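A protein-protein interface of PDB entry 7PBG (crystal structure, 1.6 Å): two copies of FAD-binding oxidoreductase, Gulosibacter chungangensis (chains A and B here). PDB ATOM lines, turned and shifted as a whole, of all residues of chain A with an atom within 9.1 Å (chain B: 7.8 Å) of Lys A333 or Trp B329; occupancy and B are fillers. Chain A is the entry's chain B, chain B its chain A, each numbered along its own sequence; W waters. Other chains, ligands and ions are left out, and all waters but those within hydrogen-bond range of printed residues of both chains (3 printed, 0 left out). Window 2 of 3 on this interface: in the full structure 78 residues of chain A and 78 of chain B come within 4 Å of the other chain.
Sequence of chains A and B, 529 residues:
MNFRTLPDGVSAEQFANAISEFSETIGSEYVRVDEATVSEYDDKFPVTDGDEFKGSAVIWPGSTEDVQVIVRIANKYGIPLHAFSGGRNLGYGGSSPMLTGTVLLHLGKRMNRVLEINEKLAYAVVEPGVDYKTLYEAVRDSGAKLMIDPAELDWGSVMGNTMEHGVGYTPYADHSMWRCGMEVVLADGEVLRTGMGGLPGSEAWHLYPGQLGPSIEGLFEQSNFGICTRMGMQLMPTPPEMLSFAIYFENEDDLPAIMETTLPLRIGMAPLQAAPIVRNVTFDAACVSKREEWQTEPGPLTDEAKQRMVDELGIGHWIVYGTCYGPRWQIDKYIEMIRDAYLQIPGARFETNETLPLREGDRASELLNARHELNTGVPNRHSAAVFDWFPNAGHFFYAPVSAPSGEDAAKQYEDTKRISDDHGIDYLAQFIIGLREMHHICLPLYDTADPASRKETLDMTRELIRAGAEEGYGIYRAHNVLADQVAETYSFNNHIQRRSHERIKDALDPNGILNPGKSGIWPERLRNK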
ATOM      1  N   LEU A 243     -35.459 -25.829  -1.943  1.00  0.00           N
ATOM      2  CA  LEU A 243     -36.212 -26.848  -2.701  1.00  0.00           C
ATOM      3  C   LEU A 243     -36.507 -28.036  -1.798  1.00  0.00           C
ATOM      4  O   LEU A 243     -35.597 -28.550  -1.200  1.00  0.00           O
ATOM      5  CB  LEU A 243     -35.388 -27.283  -3.905  1.00  0.00           C
ATOM      6  CG  LEU A 243     -36.137 -28.178  -4.885  1.00  0.00           C
ATOM      7  CD1 LEU A 243     -37.309 -27.448  -5.510  1.00  0.00           C
ATOM      8  CD2 LEU A 243     -35.169 -28.613  -5.956  1.00  0.00           C
ATOM      9  N   LEU A 265     -25.870 -39.455   4.949  1.00  0.00           N
ATOM     10  CA  LEU A 265     -26.194 -38.236   4.181  1.00  0.00           C
ATOM     11  C   LEU A 265     -26.454 -37.045   5.097  1.00  0.00           C
ATOM     12  O   LEU A 265     -26.485 -35.885   4.600  1.00  0.00           O
ATOM     13  CB  LEU A 265     -27.436 -38.487   3.339  1.00  0.00           C
ATOM     14  CG  LEU A 265     -27.304 -39.593   2.312  1.00  0.00           C
ATOM     15  CD1 LEU A 265     -28.670 -39.850   1.668  1.00  0.00           C
ATOM     16  CD2 LEU A 265     -26.244 -39.255   1.248  1.00  0.00           C
ATOM     17  N   ALA A 270     -24.534 -32.429   5.134  1.00  0.00           N
ATOM     18  CA  ALA A 270     -24.716 -32.323   3.668  1.00  0.00           C
ATOM     19  C   ALA A 270     -24.617 -33.723   3.107  1.00  0.00           C
ATOM     20  O   ALA A 270     -23.773 -34.479   3.548  1.00  0.00           O
ATOM     21  CB  ALA A 270     -23.645 -31.423   3.086  1.00  0.00           C
ATOM     22  N   PRO A 271     -25.422 -34.138   2.108  1.00  0.00           N
ATOM     23  CA  PRO A 271     -26.416 -33.287   1.448  1.00  0.00           C
ATOM     24  C   PRO A 271     -27.747 -33.046   2.169  1.00  0.00           C
ATOM     25  O   PRO A 271     -28.499 -32.133   1.769  1.00  0.00           O
ATOM     26  CB  PRO A 271     -26.680 -34.086   0.160  1.00  0.00           C
ATOM     27  CG  PRO A 271     -26.505 -35.507   0.587  1.00  0.00           C
ATOM     28  CD  PRO A 271     -25.301 -35.462   1.498  1.00  0.00           C
ATOM     29  N   LEU A 272     -27.966 -33.737   3.298  1.00  0.00           N
ATOM     30  CA  LEU A 272     -29.117 -33.448   4.188  1.00  0.00           C
ATOM     31  C   LEU A 272     -28.716 -32.326   5.159  1.00  0.00           C
ATOM     32  O   LEU A 272     -28.208 -32.591   6.283  1.00  0.00           O
ATOM     33  CB  LEU A 272     -29.579 -34.737   4.877  1.00  0.00           C
ATOM     34  CG  LEU A 272     -30.220 -35.817   3.984  1.00  0.00           C
ATOM     35  CD1 LEU A 272     -30.481 -37.096   4.752  1.00  0.00           C
ATOM     36  CD2 LEU A 272     -31.514 -35.298   3.346  1.00  0.00           C
ATOM     37  N   GLN A 273     -29.058 -31.102   4.767  1.00  0.00           N
ATOM     38  CA  GLN A 273     -28.725 -29.846   5.486  1.00  0.00           C
ATOM     39  C   GLN A 273     -29.648 -29.615   6.670  1.00  0.00           C
ATOM     40  O   GLN A 273     -29.296 -28.816   7.522  1.00  0.00           O
ATOM     41  CB  GLN A 273     -28.897 -28.687   4.537  1.00  0.00           C
ATOM     42  CG  GLN A 273     -27.854 -28.731   3.454  1.00  0.00           C
ATOM     43  CD  GLN A 273     -28.204 -27.747   2.370  1.00  0.00           C
ATOM     44  OE1 GLN A 273     -29.106 -28.012   1.592  1.00  0.00           O
ATOM     45  NE2 GLN A 273     -27.423 -26.701   2.287  1.00  0.00           N
ATOM     46  N   CYS A 324     -33.484 -28.850   0.713  1.00  0.00           N
ATOM     47  CA  CYS A 324     -32.136 -28.343   0.432  1.00  0.00           C
ATOM     48  C   CYS A 324     -32.183 -26.822   0.321  1.00  0.00           C
ATOM     49  O   CYS A 324     -33.237 -26.208  -0.057  1.00  0.00           O
ATOM     50  CB  CYS A 324     -31.600 -28.956  -0.845  1.00  0.00           C
ATOM     51  SG  CYS A 324     -31.195 -30.703  -0.671  1.00  0.00           S
ATOM     52  N   TYR A 325     -31.078 -26.210   0.732  1.00  0.00           N
ATOM     53  CA  TYR A 325     -30.945 -24.760   0.920  1.00  0.00           C
ATOM     54  C   TYR A 325     -29.647 -24.255   0.274  1.00  0.00           C
ATOM     55  O   TYR A 325     -28.576 -24.919   0.398  1.00  0.00           O
ATOM     56  CB  TYR A 325     -30.813 -24.455   2.415  1.00  0.00           C
ATOM     57  CG  TYR A 325     -31.900 -25.017   3.289  1.00  0.00           C
ATOM     58  CD1 TYR A 325     -32.987 -24.219   3.634  1.00  0.00           C
ATOM     59  CD2 TYR A 325     -31.933 -26.339   3.705  1.00  0.00           C
ATOM     60  CE1 TYR A 325     -34.034 -24.704   4.406  1.00  0.00           C
ATOM     61  CE2 TYR A 325     -32.982 -26.844   4.447  1.00  0.00           C
ATOM     62  CZ  TYR A 325     -34.056 -26.017   4.804  1.00  0.00           C
ATOM     63  OH  TYR A 325     -35.093 -26.551   5.543  1.00  0.00           O
ATOM     64  N   PRO A 327     -27.701 -21.565  -3.019  1.00  0.00           N
ATOM     65  CA  PRO A 327     -27.838 -21.293  -4.442  1.00  0.00           C
ATOM     66  C   PRO A 327     -28.227 -22.559  -5.195  1.00  0.00           C
ATOM     67  O   PRO A 327     -27.924 -23.673  -4.757  1.00  0.00           O
ATOM     68  CB  PRO A 327     -26.454 -20.801  -4.855  1.00  0.00           C
ATOM     69  CG  PRO A 327     -25.545 -21.215  -3.774  1.00  0.00           C
ATOM     70  CD  PRO A 327     -26.346 -21.373  -2.507  1.00  0.00           C
ATOM     71  N   ARG A 328     -28.849 -22.371  -6.367  1.00  0.00           N
ATOM     72  CA  ARG A 328     -29.318 -23.493  -7.194  1.00  0.00           C
ATOM     73  C   ARG A 328     -28.176 -24.468  -7.498  1.00  0.00           C
ATOM     74  O   ARG A 328     -28.446 -25.676  -7.519  1.00  0.00           O
ATOM     75  CB  ARG A 328     -30.002 -23.001  -8.473  1.00  0.00           C
ATOM     76  CG  ARG A 328     -30.887 -24.063  -9.115  1.00  0.00           C
ATOM     77  CD  ARG A 328     -32.008 -24.537  -8.203  1.00  0.00           C
ATOM     78  NE  ARG A 328     -32.691 -25.682  -8.761  1.00  0.00           N
ATOM     79  CZ  ARG A 328     -34.015 -25.844  -8.780  1.00  0.00           C
ATOM     80  NH1 ARG A 328     -34.815 -24.914  -8.292  1.00  0.00           N
ATOM     81  NH2 ARG A 328     -34.518 -26.914  -9.350  1.00  0.00           N
ATOM     82  N   TRP A 329     -26.952 -23.994  -7.756  1.00  0.00           N
ATOM     83  CA  TRP A 329     -25.828 -24.916  -8.098  1.00  0.00           C
ATOM     84  C   TRP A 329     -25.589 -25.927  -6.975  1.00  0.00           C
ATOM     85  O   TRP A 329     -25.178 -27.072  -7.260  1.00  0.00           O
ATOM     86  CB  TRP A 329     -24.559 -24.171  -8.518  1.00  0.00           C
ATOM     87  CG  TRP A 329     -24.014 -23.210  -7.505  1.00  0.00           C
ATOM     88  CD1 TRP A 329     -24.172 -21.861  -7.538  1.00  0.00           C
ATOM     89  CD2 TRP A 329     -23.178 -23.494  -6.367  1.00  0.00           C
ATOM     90  NE1 TRP A 329     -23.532 -21.284  -6.475  1.00  0.00           N
ATOM     91  CE2 TRP A 329     -22.902 -22.256  -5.750  1.00  0.00           C
ATOM     92  CE3 TRP A 329     -22.646 -24.654  -5.787  1.00  0.00           C
ATOM     93  CZ2 TRP A 329     -22.159 -22.146  -4.576  1.00  0.00           C
ATOM     94  CZ3 TRP A 329     -21.897 -24.545  -4.632  1.00  0.00           C
ATOM     95  CH2 TRP A 329     -21.666 -23.312  -4.035  1.00  0.00           C
ATOM     96  N   GLN A 330     -25.758 -25.500  -5.718  1.00  0.00           N
ATOM     97  CA  GLN A 330     -25.526 -26.370  -4.550  1.00  0.00           C
ATOM     98  C   GLN A 330     -26.758 -27.276  -4.369  1.00  0.00           C
ATOM     99  O   GLN A 330     -26.602 -28.477  -4.203  1.00  0.00           O
ATOM    100  CB  GLN A 330     -25.224 -25.515  -3.323  1.00  0.00           C
ATOM    101  CG  GLN A 330     -24.992 -26.346  -2.072  1.00  0.00           C
ATOM    102  CD  GLN A 330     -24.878 -25.490  -0.839  1.00  0.00           C
ATOM    103  OE1 GLN A 330     -25.345 -24.367  -0.810  1.00  0.00           O
ATOM    104  NE2 GLN A 330     -24.285 -26.021   0.206  1.00  0.00           N
ATOM    105  N   ILE A 331     -27.948 -26.700  -4.388  1.00  0.00           N
ATOM    106  CA  ILE A 331     -29.202 -27.482  -4.295  1.00  0.00           C
ATOM    107  C   ILE A 331     -29.143 -28.614  -5.317  1.00  0.00           C
ATOM    108  O   ILE A 331     -29.441 -29.754  -4.985  1.00  0.00           O
ATOM    109  CB  ILE A 331     -30.432 -26.597  -4.518  1.00  0.00           C
ATOM    110  CG1 ILE A 331     -30.628 -25.646  -3.345  1.00  0.00           C
ATOM    111  CG2 ILE A 331     -31.649 -27.472  -4.783  1.00  0.00           C
ATOM    112  CD1 ILE A 331     -31.783 -24.661  -3.516  1.00  0.00           C
ATOM    113  N   ASP A 332     -28.812 -28.309  -6.578  1.00  0.00           N
ATOM    114  CA  ASP A 332     -28.972 -29.353  -7.612  1.00  0.00           C
ATOM    115  C   ASP A 332     -28.015 -30.515  -7.320  1.00  0.00           C
ATOM    116  O   ASP A 332     -28.387 -31.695  -7.574  1.00  0.00           O
ATOM    117  CB  ASP A 332     -28.738 -28.783  -9.002  1.00  0.00           C
ATOM    118  CG  ASP A 332     -29.842 -27.860  -9.491  1.00  0.00           C
ATOM    119  OD1 ASP A 332     -30.968 -27.908  -8.964  1.00  0.00           O
ATOM    120  OD2 ASP A 332     -29.550 -27.087 -10.420  1.00  0.00           O
ATOM    121  N   LYS A 333     -26.816 -30.210  -6.796  1.00  0.00           N
ATOM    122  CA  LYS A 333     -25.820 -31.230  -6.432  1.00  0.00           C
ATOM    123  C   LYS A 333     -26.388 -32.086  -5.303  1.00  0.00           C
ATOM    124  O   LYS A 333     -26.305 -33.293  -5.357  1.00  0.00           O
ATOM    125  CB  LYS A 333     -24.514 -30.553  -6.010  1.00  0.00           C
ATOM    126  CG  LYS A 333     -23.712 -30.093  -7.215  1.00  0.00           C
ATOM    127  CD  LYS A 333     -22.929 -31.242  -7.824  1.00  0.00           C
ATOM    128  CE  LYS A 333     -21.981 -30.816  -8.922  1.00  0.00           C
ATOM    129  NZ  LYS A 333     -21.326 -32.026  -9.470  1.00  0.00           N
ATOM    130  N   TYR A 334     -26.936 -31.451  -4.285  1.00  0.00           N
ATOM    131  CA  TYR A 334     -27.426 -32.180  -3.101  1.00  0.00           C
ATOM    132  C   TYR A 334     -28.633 -33.025  -3.483  1.00  0.00           C
ATOM    133  O   TYR A 334     -28.678 -34.182  -3.122  1.00  0.00           O
ATOM    134  CB  TYR A 334     -27.722 -31.227  -1.955  1.00  0.00           C
ATOM    135  CG  TYR A 334     -26.512 -30.608  -1.321  1.00  0.00           C
ATOM    136  CD1 TYR A 334     -25.222 -31.060  -1.573  1.00  0.00           C
ATOM    137  CD2 TYR A 334     -26.678 -29.626  -0.378  1.00  0.00           C
ATOM    138  CE1 TYR A 334     -24.124 -30.479  -0.958  1.00  0.00           C
ATOM    139  CE2 TYR A 334     -25.600 -29.033   0.243  1.00  0.00           C
ATOM    140  CZ  TYR A 334     -24.313 -29.463  -0.038  1.00  0.00           C
ATOM    141  OH  TYR A 334     -23.288 -28.855   0.638  1.00  0.00           O
ATOM    142  N   ILE A 335     -29.602 -32.444  -4.200  1.00  0.00           N
ATOM    143  CA  ILE A 335     -30.805 -33.193  -4.646  1.00  0.00           C
ATOM    144  C   ILE A 335     -30.359 -34.437  -5.430  1.00  0.00           C
ATOM    145  O   ILE A 335     -30.962 -35.479  -5.264  1.00  0.00           O
ATOM    146  CB  ILE A 335     -31.730 -32.291  -5.469  1.00  0.00           C
ATOM    147  CG1 ILE A 335     -32.393 -31.233  -4.584  1.00  0.00           C
ATOM    148  CG2 ILE A 335     -32.731 -33.141  -6.248  1.00  0.00           C
ATOM    149  CD1 ILE A 335     -33.517 -31.740  -3.697  1.00  0.00           C
ATOM    150  N   GLU A 336     -29.416 -34.323  -6.361  1.00  0.00           N
ATOM    151  CA  GLU A 336     -28.940 -35.517  -7.094  1.00  0.00           C
ATOM    152  C   GLU A 336     -28.342 -36.537  -6.114  1.00  0.00           C
ATOM    153  O   GLU A 336     -28.695 -37.715  -6.217  1.00  0.00           O
ATOM    154  CB  GLU A 336     -27.984 -35.098  -8.215  1.00  0.00           C
ATOM    155  CG  GLU A 336     -27.084 -36.199  -8.735  1.00  0.00           C
ATOM    156  CD  GLU A 336     -26.131 -35.691  -9.804  1.00  0.00           C
ATOM    157  OE1 GLU A 336     -25.289 -34.793  -9.480  1.00  0.00           O
ATOM    158  OE2 GLU A 336     -26.241 -36.167 -10.963  1.00  0.00           O
ATOM    159  N   MET A 337     -27.562 -36.133  -5.108  1.00  0.00           N
ATOM    160  CA  MET A 337     -26.960 -37.143  -4.200  1.00  0.00           C
ATOM    161  C   MET A 337     -28.086 -37.852  -3.436  1.00  0.00           C
ATOM    162  O   MET A 337     -28.021 -39.066  -3.277  1.00  0.00           O
ATOM    163  CB  MET A 337     -26.019 -36.503  -3.182  1.00  0.00           C
ATOM    164  CG  MET A 337     -24.897 -35.776  -3.814  1.00  0.00           C
ATOM    165  SD  MET A 337     -23.962 -34.865  -2.547  1.00  0.00           S
ATOM    166  CE  MET A 337     -22.849 -33.958  -3.608  1.00  0.00           C
ATOM    167  N   ILE A 338     -29.079 -37.092  -2.977  1.00  0.00           N
ATOM    168  CA  ILE A 338     -30.202 -37.614  -2.159  1.00  0.00           C
ATOM    169  C   ILE A 338     -31.052 -38.565  -3.017  1.00  0.00           C
ATOM    170  O   ILE A 338     -31.319 -39.707  -2.593  1.00  0.00           O
ATOM    171  CB  ILE A 338     -31.037 -36.460  -1.573  1.00  0.00           C
ATOM    172  CG1 ILE A 338     -30.246 -35.623  -0.572  1.00  0.00           C
ATOM    173  CG2 ILE A 338     -32.329 -36.975  -0.977  1.00  0.00           C
ATOM    174  CD1 ILE A 338     -30.860 -34.261  -0.334  1.00  0.00           C
ATOM    175  N   ARG A 339     -31.482 -38.099  -4.187  1.00  0.00           N
ATOM    176  CA  ARG A 339     -32.315 -38.919  -5.101  1.00  0.00           C
ATOM    177  C   ARG A 339     -31.565 -40.219  -5.396  1.00  0.00           C
ATOM    178  O   ARG A 339     -32.166 -41.332  -5.195  1.00  0.00           O
ATOM    179  CB  ARG A 339     -32.604 -38.132  -6.375  1.00  0.00           C
ATOM    180  CG  ARG A 339     -33.586 -38.822  -7.304  1.00  0.00           C
ATOM    181  CD  ARG A 339     -33.758 -37.957  -8.544  1.00  0.00           C
ATOM    182  NE  ARG A 339     -34.896 -38.427  -9.299  1.00  0.00           N
ATOM    183  CZ  ARG A 339     -34.908 -39.492 -10.101  1.00  0.00           C
ATOM    184  NH1 ARG A 339     -33.822 -40.222 -10.295  1.00  0.00           N
ATOM    185  NH2 ARG A 339     -36.031 -39.814 -10.722  1.00  0.00           N
ATOM    186  N   ASP A 340     -30.281 -40.113  -5.788  1.00  0.00           N
ATOM    187  CA  ASP A 340     -29.486 -41.315  -6.169  1.00  0.00           C
ATOM    188  C   ASP A 340     -29.429 -42.299  -4.994  1.00  0.00           C
ATOM    189  O   ASP A 340     -29.566 -43.497  -5.215  1.00  0.00           O
ATOM    190  CB  ASP A 340     -28.054 -40.996  -6.625  1.00  0.00           C
ATOM    191  CG  ASP A 340     -27.927 -40.310  -7.985  1.00  0.00           C
ATOM    192  OD1 ASP A 340     -28.960 -40.119  -8.654  1.00  0.00           O
ATOM    193  OD2 ASP A 340     -26.785 -39.947  -8.356  1.00  0.00           O
ATOM    194  N   PRO B 240     -14.570 -34.341   1.555  1.00  0.00           N
ATOM    195  CA  PRO B 240     -13.745 -34.803   0.443  1.00  0.00           C
ATOM    196  C   PRO B 240     -12.411 -34.049   0.267  1.00  0.00           C
ATOM    197  O   PRO B 240     -11.356 -34.650  -0.019  1.00  0.00           O
ATOM    198  CB  PRO B 240     -14.651 -34.571  -0.778  1.00  0.00           C
ATOM    199  CG  PRO B 240     -16.048 -34.497  -0.245  1.00  0.00           C
ATOM    200  CD  PRO B 240     -15.956 -34.053   1.210  1.00  0.00           C
ATOM    201  N   GLU B 241     -12.448 -32.727   0.444  1.00  0.00           N
ATOM    202  CA  GLU B 241     -11.280 -31.842   0.279  1.00  0.00           C
ATOM    203  C   GLU B 241     -11.355 -30.693   1.262  1.00  0.00           C
ATOM    204  O   GLU B 241     -12.465 -30.390   1.714  1.00  0.00           O
ATOM    205  CB  GLU B 241     -11.274 -31.301  -1.154  1.00  0.00           C
ATOM    206  CG  GLU B 241      -9.936 -30.871  -1.630  1.00  0.00           C
ATOM    207  CD  GLU B 241      -9.737 -30.918  -3.143  1.00  0.00           C
ATOM    208  OE1 GLU B 241     -10.505 -31.561  -3.881  1.00  0.00           O
ATOM    209  OE2 GLU B 241      -8.788 -30.329  -3.549  1.00  0.00           O
ATOM    210  N   GLY B 326     -15.183 -29.361   1.612  1.00  0.00           N
ATOM    211  CA  GLY B 326     -16.216 -30.087   0.855  1.00  0.00           C
ATOM    212  C   GLY B 326     -15.640 -30.631  -0.431  1.00  0.00           C
ATOM    213  O   GLY B 326     -14.434 -30.638  -0.607  1.00  0.00           O
ATOM    214  N   PRO B 327     -16.520 -31.021  -1.363  1.00  0.00           N
ATOM    215  CA  PRO B 327     -16.064 -31.357  -2.696  1.00  0.00           C
ATOM    216  C   PRO B 327     -15.507 -30.099  -3.358  1.00  0.00           C
ATOM    217  O   PRO B 327     -15.940 -28.978  -3.044  1.00  0.00           O
ATOM    218  CB  PRO B 327     -17.326 -31.843  -3.405  1.00  0.00           C
ATOM    219  CG  PRO B 327     -18.464 -31.220  -2.661  1.00  0.00           C
ATOM    220  CD  PRO B 327     -17.982 -30.918  -1.244  1.00  0.00           C
ATOM    221  N   ARG B 328     -14.613 -30.292  -4.316  1.00  0.00           N
ATOM    222  CA  ARG B 328     -13.936 -29.170  -4.994  1.00  0.00           C
ATOM    223  C   ARG B 328     -14.938 -28.211  -5.648  1.00  0.00           C
ATOM    224  O   ARG B 328     -14.658 -26.993  -5.644  1.00  0.00           O
ATOM    225  CB  ARG B 328     -12.895 -29.666  -5.989  1.00  0.00           C
ATOM    226  CG  ARG B 328     -11.875 -28.613  -6.380  1.00  0.00           C
ATOM    227  CD  ARG B 328     -11.073 -28.039  -5.229  1.00  0.00           C
ATOM    228  NE  ARG B 328     -10.203 -26.953  -5.660  1.00  0.00           N
ATOM    229  CZ  ARG B 328      -8.891 -26.819  -5.391  1.00  0.00           C
ATOM    230  NH1 ARG B 328      -8.249 -27.677  -4.598  1.00  0.00           N
ATOM    231  NH2 ARG B 328      -8.254 -25.762  -5.882  1.00  0.00           N
ATOM    232  N   TRP B 329     -16.063 -28.695  -6.200  1.00  0.00           N
ATOM    233  CA  TRP B 329     -17.050 -27.788  -6.856  1.00  0.00           C
ATOM    234  C   TRP B 329     -17.548 -26.754  -5.868  1.00  0.00           C
ATOM    235  O   TRP B 329     -17.786 -25.607  -6.274  1.00  0.00           O
ATOM    236  CB  TRP B 329     -18.218 -28.526  -7.540  1.00  0.00           C
ATOM    237  CG  TRP B 329     -18.947 -29.514  -6.685  1.00  0.00           C
ATOM    238  CD1 TRP B 329     -18.785 -30.872  -6.644  1.00  0.00           C
ATOM    239  CD2 TRP B 329     -20.033 -29.217  -5.804  1.00  0.00           C
ATOM    240  NE1 TRP B 329     -19.639 -31.423  -5.727  1.00  0.00           N
ATOM    241  CE2 TRP B 329     -20.442 -30.442  -5.228  1.00  0.00           C
ATOM    242  CE3 TRP B 329     -20.718 -28.046  -5.464  1.00  0.00           C
ATOM    243  CZ2 TRP B 329     -21.434 -30.500  -4.259  1.00  0.00           C
ATOM    244  CZ3 TRP B 329     -21.724 -28.126  -4.534  1.00  0.00           C
ATOM    245  CH2 TRP B 329     -22.067 -29.331  -3.942  1.00  0.00           C
ATOM    246  N   GLN B 330     -17.712 -27.155  -4.616  1.00  0.00           N
ATOM    247  CA  GLN B 330     -18.199 -26.264  -3.546  1.00  0.00           C
ATOM    248  C   GLN B 330     -17.061 -25.350  -3.068  1.00  0.00           C
ATOM    249  O   GLN B 330     -17.252 -24.119  -2.959  1.00  0.00           O
ATOM    250  CB  GLN B 330     -18.697 -27.119  -2.382  1.00  0.00           C
ATOM    251  CG  GLN B 330     -19.202 -26.267  -1.226  1.00  0.00           C
ATOM    252  CD  GLN B 330     -19.749 -27.119  -0.109  1.00  0.00           C
ATOM    253  OE1 GLN B 330     -19.347 -28.266   0.086  1.00  0.00           O
ATOM    254  NE2 GLN B 330     -20.702 -26.553   0.607  1.00  0.00           N
ATOM    255  N   ILE B 331     -15.904 -25.926  -2.767  1.00  0.00           N
ATOM    256  CA  ILE B 331     -14.718 -25.111  -2.370  1.00  0.00           C
ATOM    257  C   ILE B 331     -14.458 -24.021  -3.393  1.00  0.00           C
ATOM    258  O   ILE B 331     -14.239 -22.864  -2.993  1.00  0.00           O
ATOM    259  CB  ILE B 331     -13.475 -25.996  -2.151  1.00  0.00           C
ATOM    260  CG1 ILE B 331     -13.647 -26.885  -0.922  1.00  0.00           C
ATOM    261  CG2 ILE B 331     -12.237 -25.113  -2.097  1.00  0.00           C
ATOM    262  CD1 ILE B 331     -12.565 -27.939  -0.761  1.00  0.00           C
ATOM    263  N   ASP B 332     -14.461 -24.336  -4.677  1.00  0.00           N
ATOM    264  CA  ASP B 332     -14.048 -23.334  -5.677  1.00  0.00           C
ATOM    265  C   ASP B 332     -15.051 -22.170  -5.676  1.00  0.00           C
ATOM    266  O   ASP B 332     -14.599 -21.017  -5.885  1.00  0.00           O
ATOM    267  CB  ASP B 332     -13.962 -23.973  -7.059  1.00  0.00           C
ATOM    268  CG  ASP B 332     -12.737 -24.852  -7.232  1.00  0.00           C
ATOM    269  OD1 ASP B 332     -11.859 -24.882  -6.307  1.00  0.00           O
ATOM    270  OD2 ASP B 332     -12.672 -25.512  -8.273  1.00  0.00           O
ATOM    271  N   LYS B 333     -16.343 -22.450  -5.495  1.00  0.00           N
ATOM    272  CA  LYS B 333     -17.380 -21.385  -5.410  1.00  0.00           C
ATOM    273  C   LYS B 333     -17.135 -20.539  -4.171  1.00  0.00           C
ATOM    274  O   LYS B 333     -17.217 -19.322  -4.258  1.00  0.00           O
ATOM    275  CB  LYS B 333     -18.766 -22.002  -5.351  1.00  0.00           C
ATOM    276  CG  LYS B 333     -19.220 -22.609  -6.666  1.00  0.00           C
ATOM    277  CD  LYS B 333     -19.754 -21.559  -7.603  1.00  0.00           C
ATOM    278  CE  LYS B 333     -20.567 -22.164  -8.720  1.00  0.00           C
ATOM    279  NZ  LYS B 333     -20.733 -21.163  -9.791  1.00  0.00           N
ATOM    280  N   TYR B 334     -16.902 -21.156  -3.029  1.00  0.00           N
ATOM    281  CA  TYR B 334     -16.731 -20.346  -1.805  1.00  0.00           C
ATOM    282  C   TYR B 334     -15.458 -19.503  -1.885  1.00  0.00           C
ATOM    283  O   TYR B 334     -15.475 -18.332  -1.508  1.00  0.00           O
ATOM    284  CB  TYR B 334     -16.791 -21.236  -0.561  1.00  0.00           C
ATOM    285  CG  TYR B 334     -18.123 -21.862  -0.245  1.00  0.00           C
ATOM    286  CD1 TYR B 334     -19.304 -21.508  -0.893  1.00  0.00           C
ATOM    287  CD2 TYR B 334     -18.223 -22.795   0.782  1.00  0.00           C
ATOM    288  CE1 TYR B 334     -20.510 -22.114  -0.577  1.00  0.00           C
ATOM    289  CE2 TYR B 334     -19.421 -23.407   1.105  1.00  0.00           C
ATOM    290  CZ  TYR B 334     -20.581 -23.041   0.443  1.00  0.00           C
ATOM    291  OH  TYR B 334     -21.793 -23.595   0.758  1.00  0.00           O
ATOM    292  N   ILE B 335     -14.348 -20.098  -2.313  1.00  0.00           N
ATOM    293  CA  ILE B 335     -13.064 -19.365  -2.424  1.00  0.00           C
ATOM    294  C   ILE B 335     -13.256 -18.165  -3.349  1.00  0.00           C
ATOM    295  O   ILE B 335     -12.845 -17.090  -2.998  1.00  0.00           O
ATOM    296  CB  ILE B 335     -11.961 -20.319  -2.910  1.00  0.00           C
ATOM    297  CG1 ILE B 335     -11.645 -21.375  -1.853  1.00  0.00           C
ATOM    298  CG2 ILE B 335     -10.759 -19.530  -3.415  1.00  0.00           C
ATOM    299  CD1 ILE B 335     -10.834 -20.870  -0.689  1.00  0.00           C
HETATM  300  O   HOH W   1     -21.182 -28.382   3.378  1.00  0.00           O
HETATM  301  O   HOH W   2     -21.278 -30.200   0.461  1.00  0.00           O
HETATM  302  O   HOH W   3     -23.747 -22.297   0.036  1.00  0.00           O
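The side-chain amide nitrogen of Gln B330 is in hydrogen-bond range of the side-chain hydroxyl of Tyr A334 (3.5 Å).
The side-chain amide nitrogen (NE2) of Gln B330 is in hydrogen-bond range of the side-chain hydroxyl (OH) of Tyr B334 (3.2 Å).
The backbone carbonyl oxygen of Tyr A325 lies close to the side-chain amide oxygen of Gln A330 (3.5 Å).
The side-chain amide nitrogen (NE2) of Gln A330 sits at hydrogen-bond distance from the side-chain hydroxyl (OH) of Tyr A334, at 3.0 Å.
Among the printed residues, pairs that only touch across the chains: Trp A329 with Trp B329 (3.6 Å), Trp A329 with Lys B333 (3.4 Å), Trp A329 with Tyr B334 (3.8 Å), Gln A330 with Gln B330 (3.6 Å), Gln A330 with Tyr B334 (3.5 Å), Lys A333 with Trp B329 (3.4 Å), Tyr A334 with Trp B329 (3.8 Å) and Met A337 with Trp B329 (3.8 Å).
Lys A333 touches one residue of chain B.
Of chain A, only Trp A329, Lys A333, Tyr A334 and Met A337 come within 4 Å of Trp B329.
Of the printed residues of chain B, Met A337 touches Trp B329.
Printed residues of chain B within 4 Å of Tyr A334: Trp B329 and Gln B330.
Printed residues of chain A within 4 Å of Tyr B334: Trp A329 (3.8 Å) and Gln A330 (3.5 Å).
Asp B332 touches none of the printed residues of chain A.
Arg A339 touches none of the printed residues of chain B.
The nearest printed residue of chain B that does not touch Trp A329 is Gln B330 (4.2 Å).
Of the 22 printed residues of chain A, 5 touch a printed residue of chain B.
Of the 12 printed residues of chain B, 4 touch a printed residue of chain A.
Hydrophobic or aromatic side chains of chain B that line the printed part of chain A: Trp B329 and Tyr B334.
Trp B329 touches its own counterpart, Trp A329.
Trp A329 touches Tyr B334, and with the chains exchanged Tyr A334 touches Trp B329.
Gln B330 touches its own counterpart, Gln A330.
Gln A330 touches Tyr B334, and with the chains exchanged Tyr A334 touches Gln B330.
Of the 9 pairs that touch across the chains among the printed residues, 8 have their exchanged pair printed and touching as well.
Water W2 lies within hydrogen-bond range of the side-chain hydroxyl of Tyr A334 (2.4 Å) and the side-chain amide oxygen of Gln B330 (2.8 Å).
Water W3 lies within hydrogen-bond range of the side-chain hydroxyl of Tyr B334 (2.5 Å) and the side-chain amide oxygen of Gln A330 (2.7 Å).
Water W1 lies within hydrogen-bond range of the side-chain amide nitrogen of Gln B330 (3.4 Å) and the side-chain hydroxyl of Tyr A334 (3.5 Å).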
